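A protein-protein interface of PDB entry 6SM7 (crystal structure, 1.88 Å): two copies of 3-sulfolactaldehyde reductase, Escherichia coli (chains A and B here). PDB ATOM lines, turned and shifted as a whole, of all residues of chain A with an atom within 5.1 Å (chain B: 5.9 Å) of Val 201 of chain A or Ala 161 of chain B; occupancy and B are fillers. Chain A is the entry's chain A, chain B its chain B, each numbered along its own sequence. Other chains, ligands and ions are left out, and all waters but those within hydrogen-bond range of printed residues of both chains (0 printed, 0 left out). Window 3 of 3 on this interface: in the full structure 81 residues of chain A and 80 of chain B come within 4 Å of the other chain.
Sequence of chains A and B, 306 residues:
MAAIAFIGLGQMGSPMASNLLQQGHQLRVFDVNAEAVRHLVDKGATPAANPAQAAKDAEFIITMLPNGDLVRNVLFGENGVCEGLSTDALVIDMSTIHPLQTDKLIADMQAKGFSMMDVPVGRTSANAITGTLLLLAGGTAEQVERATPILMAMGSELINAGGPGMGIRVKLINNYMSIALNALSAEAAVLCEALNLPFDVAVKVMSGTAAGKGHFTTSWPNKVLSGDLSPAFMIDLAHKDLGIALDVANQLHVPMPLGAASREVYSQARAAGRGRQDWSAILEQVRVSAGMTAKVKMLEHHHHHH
The backbone carbonyl oxygen (O) of Ile 159 of chain B lies within hydrogen-bond range of the backbone NH (N) of Ala 137 of chain B (2.9 Å). The backbone NH of Ala 161 of chain B is in hydrogen-bond range of the backbone carbonyl oxygen of Ala 137 of chain B.
CD1 of Leu 197 of chain A touches SD of Met 166 of chain B, 3.7 Å away. Leu 197 of chain A touches Val 170 of chain B. Ala 161 of chain B touches Val 201 of chain A (O to CG1, 3.9 Å). O of Val 201 of chain A touches CG2 of Val 170 of chain B (3.99 Å). Val 170 of chain B touches Ala 202 of chain A. Leu 136 of chain B touches Val 205 of chain A (CD2 to CG2, 3.7 Å). CG2 of Val 205 of chain A touches CD1 of Ile 159 of chain B, at 3.8 Å. Val 205 of chain A touches Val 170 of chain B (CG2 to CG2, 3.5 Å).
Of the printed residues of chain B, Leu 197 of chain A touches Met 166 (3.7 Å) and Val 170 (3.5 Å). Printed residues of chain B within 4 Å of Val 201 of chain A: Ala 161 and Val 170. Printed residues of chain A within 4 Å of Leu 136 of chain B: Val 205. Of the printed residues of chain A, Ile 159 of chain B touches Val 205 (3.8 Å). Of chain A, only Val 201 (3.9 Å) comes within 4 Å of Ala 161 of chain B. Of the printed residues of chain A, Met 166 of chain B touches Leu 197 (3.7 Å). Of the printed residues of chain A, Val 170 of chain B touches Leu 197, Val 201, Ala 202 and Val 205.
Of the 9 printed residues of chain A, 4 touch a printed residue of chain B. Along chain A the printed residues that touch a printed residue of chain B span positions 197 to 205.
No position is printed for both chains. Of the 8 pairs that touch across the chains among the printed residues, none has its exchanged pair printed and touching as well.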
ATOM      1  N   LEU A 197      -9.799  21.017 -13.200  1.00  0.00           N
ATOM      2  CA  LEU A 197     -10.935  21.020 -14.141  1.00  0.00           C
ATOM      3  C   LEU A 197     -10.570  20.067 -15.269  1.00  0.00           C
ATOM      4  O   LEU A 197      -9.557  20.278 -15.930  1.00  0.00           O
ATOM      5  CB  LEU A 197     -11.176  22.431 -14.677  1.00  0.00           C
ATOM      6  CG  LEU A 197     -12.252  22.570 -15.732  1.00  0.00           C
ATOM      7  CD1 LEU A 197     -13.626  22.310 -15.118  1.00  0.00           C
ATOM      8  CD2 LEU A 197     -12.199  23.965 -16.332  1.00  0.00           C
ATOM      9  N   PRO A 198     -11.381  19.022 -15.542  1.00  0.00           N
ATOM     10  CA  PRO A 198     -11.128  18.142 -16.679  1.00  0.00           C
ATOM     11  C   PRO A 198     -11.024  18.937 -17.984  1.00  0.00           C
ATOM     12  O   PRO A 198     -11.871  19.779 -18.285  1.00  0.00           O
ATOM     13  CB  PRO A 198     -12.347  17.189 -16.706  1.00  0.00           C
ATOM     14  CG  PRO A 198     -12.840  17.198 -15.268  1.00  0.00           C
ATOM     15  CD  PRO A 198     -12.579  18.613 -14.780  1.00  0.00           C
ATOM     16  N   PHE A 199      -9.964  18.665 -18.737  1.00  0.00           N
ATOM     17  CA  PHE A 199      -9.630  19.420 -19.966  1.00  0.00           C
ATOM     18  C   PHE A 199     -10.795  19.344 -20.963  1.00  0.00           C
ATOM     19  O   PHE A 199     -11.059  20.360 -21.635  1.00  0.00           O
ATOM     20  CB  PHE A 199      -8.332  18.892 -20.575  1.00  0.00           C
ATOM     21  CG  PHE A 199      -7.875  19.674 -21.774  1.00  0.00           C
ATOM     22  CD1 PHE A 199      -7.637  21.036 -21.676  1.00  0.00           C
ATOM     23  CD2 PHE A 199      -7.699  19.050 -23.000  1.00  0.00           C
ATOM     24  CE1 PHE A 199      -7.208  21.755 -22.778  1.00  0.00           C
ATOM     25  CE2 PHE A 199      -7.277  19.776 -24.100  1.00  0.00           C
ATOM     26  CZ  PHE A 199      -7.029  21.118 -23.980  1.00  0.00           C
ATOM     27  N   ASP A 200     -11.470  18.185 -21.094  1.00  0.00           N
ATOM     28  CA  ASP A 200     -12.555  17.977 -22.091  1.00  0.00           C
ATOM     29  C   ASP A 200     -13.664  19.014 -21.864  1.00  0.00           C
ATOM     30  O   ASP A 200     -14.279  19.466 -22.847  1.00  0.00           O
ATOM     31  CB  ASP A 200     -13.126  16.545 -22.014  1.00  0.00           C
ATOM     32  CG  ASP A 200     -14.112  16.289 -20.870  1.00  0.00           C
ATOM     33  OD1 ASP A 200     -15.316  16.593 -21.023  1.00  0.00           O
ATOM     34  OD2 ASP A 200     -13.689  15.776 -19.832  1.00  0.00           O
ATOM     35  N   VAL A 201     -13.916  19.365 -20.595  1.00  0.00           N
ATOM     36  CA  VAL A 201     -14.980  20.350 -20.232  1.00  0.00           C
ATOM     37  C   VAL A 201     -14.568  21.715 -20.784  1.00  0.00           C
ATOM     38  O   VAL A 201     -15.406  22.375 -21.416  1.00  0.00           O
ATOM     39  CB  VAL A 201     -15.214  20.397 -18.719  1.00  0.00           C
ATOM     40  CG1 VAL A 201     -16.139  21.548 -18.337  1.00  0.00           C
ATOM     41  CG2 VAL A 201     -15.725  19.052 -18.195  1.00  0.00           C
ATOM     42  N   ALA A 202     -13.313  22.109 -20.561  1.00  0.00           N
ATOM     43  CA  ALA A 202     -12.767  23.391 -21.064  1.00  0.00           C
ATOM     44  C   ALA A 202     -12.850  23.412 -22.584  1.00  0.00           C
ATOM     45  O   ALA A 202     -13.312  24.409 -23.136  1.00  0.00           O
ATOM     46  CB  ALA A 202     -11.354  23.600 -20.556  1.00  0.00           C
ATOM     47  N   VAL A 203     -12.447  22.324 -23.259  1.00  0.00           N
ATOM     48  CA  VAL A 203     -12.438  22.316 -24.751  1.00  0.00           C
ATOM     49  C   VAL A 203     -13.882  22.446 -25.264  1.00  0.00           C
ATOM     50  O   VAL A 203     -14.102  23.200 -26.242  1.00  0.00           O
ATOM     51  CB  VAL A 203     -11.735  21.077 -25.333  1.00  0.00           C
ATOM     52  CG1 VAL A 203     -11.890  21.034 -26.839  1.00  0.00           C
ATOM     53  CG2 VAL A 203     -10.267  21.067 -24.962  1.00  0.00           C
ATOM     54  N   LYS A 204     -14.837  21.775 -24.613  1.00  0.00           N
ATOM     55  CA  LYS A 204     -16.270  21.865 -25.016  1.00  0.00           C
ATOM     56  C   LYS A 204     -16.700  23.335 -24.925  1.00  0.00           C
ATOM     57  O   LYS A 204     -17.276  23.854 -25.888  1.00  0.00           O
ATOM     58  CB  LYS A 204     -17.159  20.962 -24.152  1.00  0.00           C
ATOM     59  CG  LYS A 204     -18.636  20.965 -24.557  1.00  0.00           C
ATOM     60  N   VAL A 205     -16.388  24.024 -23.826  1.00  0.00           N
ATOM     61  CA  VAL A 205     -16.805  25.452 -23.670  1.00  0.00           C
ATOM     62  C   VAL A 205     -16.087  26.305 -24.724  1.00  0.00           C
ATOM     63  O   VAL A 205     -16.747  27.085 -25.426  1.00  0.00           O
ATOM     64  CB  VAL A 205     -16.552  25.946 -22.239  1.00  0.00           C
ATOM     65  CG1 VAL A 205     -16.665  27.458 -22.106  1.00  0.00           C
ATOM     66  CG2 VAL A 205     -17.503  25.241 -21.274  1.00  0.00           C
ATOM     67  N   LEU B 136     -22.563  28.195 -17.868  1.00  0.00           N
ATOM     68  CA  LEU B 136     -21.429  27.357 -17.424  1.00  0.00           C
ATOM     69  C   LEU B 136     -21.757  26.868 -16.017  1.00  0.00           C
ATOM     70  O   LEU B 136     -21.368  27.511 -15.036  1.00  0.00           O
ATOM     71  CB  LEU B 136     -20.136  28.172 -17.523  1.00  0.00           C
ATOM     72  CG  LEU B 136     -19.908  28.828 -18.882  1.00  0.00           C
ATOM     73  CD1 LEU B 136     -18.671  29.722 -18.863  1.00  0.00           C
ATOM     74  CD2 LEU B 136     -19.807  27.798 -19.998  1.00  0.00           C
ATOM     75  N   ALA B 137     -22.507  25.759 -15.931  1.00  0.00           N
ATOM     76  CA  ALA B 137     -23.173  25.330 -14.687  1.00  0.00           C
ATOM     77  C   ALA B 137     -22.239  24.491 -13.810  1.00  0.00           C
ATOM     78  O   ALA B 137     -22.062  23.253 -14.049  1.00  0.00           O
ATOM     79  CB  ALA B 137     -24.452  24.589 -15.021  1.00  0.00           C
ATOM     80  N   GLY B 138     -21.682  25.135 -12.793  1.00  0.00           N
ATOM     81  CA  GLY B 138     -21.079  24.457 -11.642  1.00  0.00           C
ATOM     82  C   GLY B 138     -22.183  23.957 -10.736  1.00  0.00           C
ATOM     83  O   GLY B 138     -23.347  24.152 -11.078  1.00  0.00           O
ATOM     84  N   ILE B 159     -23.928  24.069 -20.297  1.00  0.00           N
ATOM     85  CA  ILE B 159     -22.840  23.072 -20.198  1.00  0.00           C
ATOM     86  C   ILE B 159     -22.694  22.694 -18.730  1.00  0.00           C
ATOM     87  O   ILE B 159     -22.609  23.574 -17.882  1.00  0.00           O
ATOM     88  CB  ILE B 159     -21.565  23.631 -20.854  1.00  0.00           C
ATOM     89  CG1 ILE B 159     -21.766  23.692 -22.373  1.00  0.00           C
ATOM     90  CG2 ILE B 159     -20.367  22.797 -20.449  1.00  0.00           C
ATOM     91  CD1 ILE B 159     -20.703  24.429 -23.147  1.00  0.00           C
ATOM     92  N   ASN B 160     -22.744  21.401 -18.440  1.00  0.00           N
ATOM     93  CA  ASN B 160     -22.554  20.893 -17.064  1.00  0.00           C
ATOM     94  C   ASN B 160     -21.050  20.836 -16.826  1.00  0.00           C
ATOM     95  O   ASN B 160     -20.387  20.001 -17.448  1.00  0.00           O
ATOM     96  CB  ASN B 160     -23.278  19.558 -16.846  1.00  0.00           C
ATOM     97  CG  ASN B 160     -23.285  19.145 -15.397  1.00  0.00           C
ATOM     98  OD1 ASN B 160     -22.248  19.198 -14.748  1.00  0.00           O
ATOM     99  ND2 ASN B 160     -24.444  18.757 -14.859  1.00  0.00           N
ATOM    100  N   ALA B 161     -20.529  21.698 -15.958  1.00  0.00           N
ATOM    101  CA  ALA B 161     -19.078  21.845 -15.732  1.00  0.00           C
ATOM    102  C   ALA B 161     -18.563  20.689 -14.875  1.00  0.00           C
ATOM    103  O   ALA B 161     -17.349  20.527 -14.801  1.00  0.00           O
ATOM    104  CB  ALA B 161     -18.778  23.193 -15.105  1.00  0.00           C
ATOM    105  N   GLY B 162     -19.457  19.968 -14.188  1.00  0.00           N
ATOM    106  CA  GLY B 162     -19.157  18.682 -13.528  1.00  0.00           C
ATOM    107  C   GLY B 162     -18.850  18.827 -12.054  1.00  0.00           C
ATOM    108  O   GLY B 162     -18.190  17.937 -11.503  1.00  0.00           O
ATOM    109  N   GLY B 163     -19.314  19.881 -11.389  1.00  0.00           N
ATOM    110  CA  GLY B 163     -19.194  19.941  -9.924  1.00  0.00           C
ATOM    111  C   GLY B 163     -19.180  21.362  -9.380  1.00  0.00           C
ATOM    112  O   GLY B 163     -19.000  22.326 -10.127  1.00  0.00           O
ATOM    113  N   MET B 166     -16.692  24.269 -10.613  1.00  0.00           N
ATOM    114  CA  MET B 166     -16.207  23.928 -11.970  1.00  0.00           C
ATOM    115  C   MET B 166     -16.754  24.938 -12.978  1.00  0.00           C
ATOM    116  O   MET B 166     -16.154  25.098 -14.056  1.00  0.00           O
ATOM    117  CB  MET B 166     -16.607  22.491 -12.353  1.00  0.00           C
ATOM    118  CG  MET B 166     -15.960  21.454 -11.454  1.00  0.00           C
ATOM    119  SD  MET B 166     -14.129  21.503 -11.589  1.00  0.00           S
ATOM    120  CE  MET B 166     -13.653  21.331  -9.869  1.00  0.00           C
ATOM    121  N   GLY B 167     -17.887  25.588 -12.683  1.00  0.00           N
ATOM    122  CA  GLY B 167     -18.424  26.590 -13.617  1.00  0.00           C
ATOM    123  C   GLY B 167     -17.512  27.802 -13.660  1.00  0.00           C
ATOM    124  O   GLY B 167     -17.173  28.271 -14.777  1.00  0.00           O
ATOM    125  N   VAL B 170     -14.170  26.920 -15.473  1.00  0.00           N
ATOM    126  CA  VAL B 170     -14.189  26.825 -16.952  1.00  0.00           C
ATOM    127  C   VAL B 170     -14.409  28.226 -17.524  1.00  0.00           C
ATOM    128  O   VAL B 170     -13.859  28.525 -18.588  1.00  0.00           O
ATOM    129  CB  VAL B 170     -15.196  25.785 -17.496  1.00  0.00           C
ATOM    130  CG1 VAL B 170     -16.647  26.245 -17.403  1.00  0.00           C
ATOM    131  CG2 VAL B 170     -14.866  25.441 -18.927  1.00  0.00           C
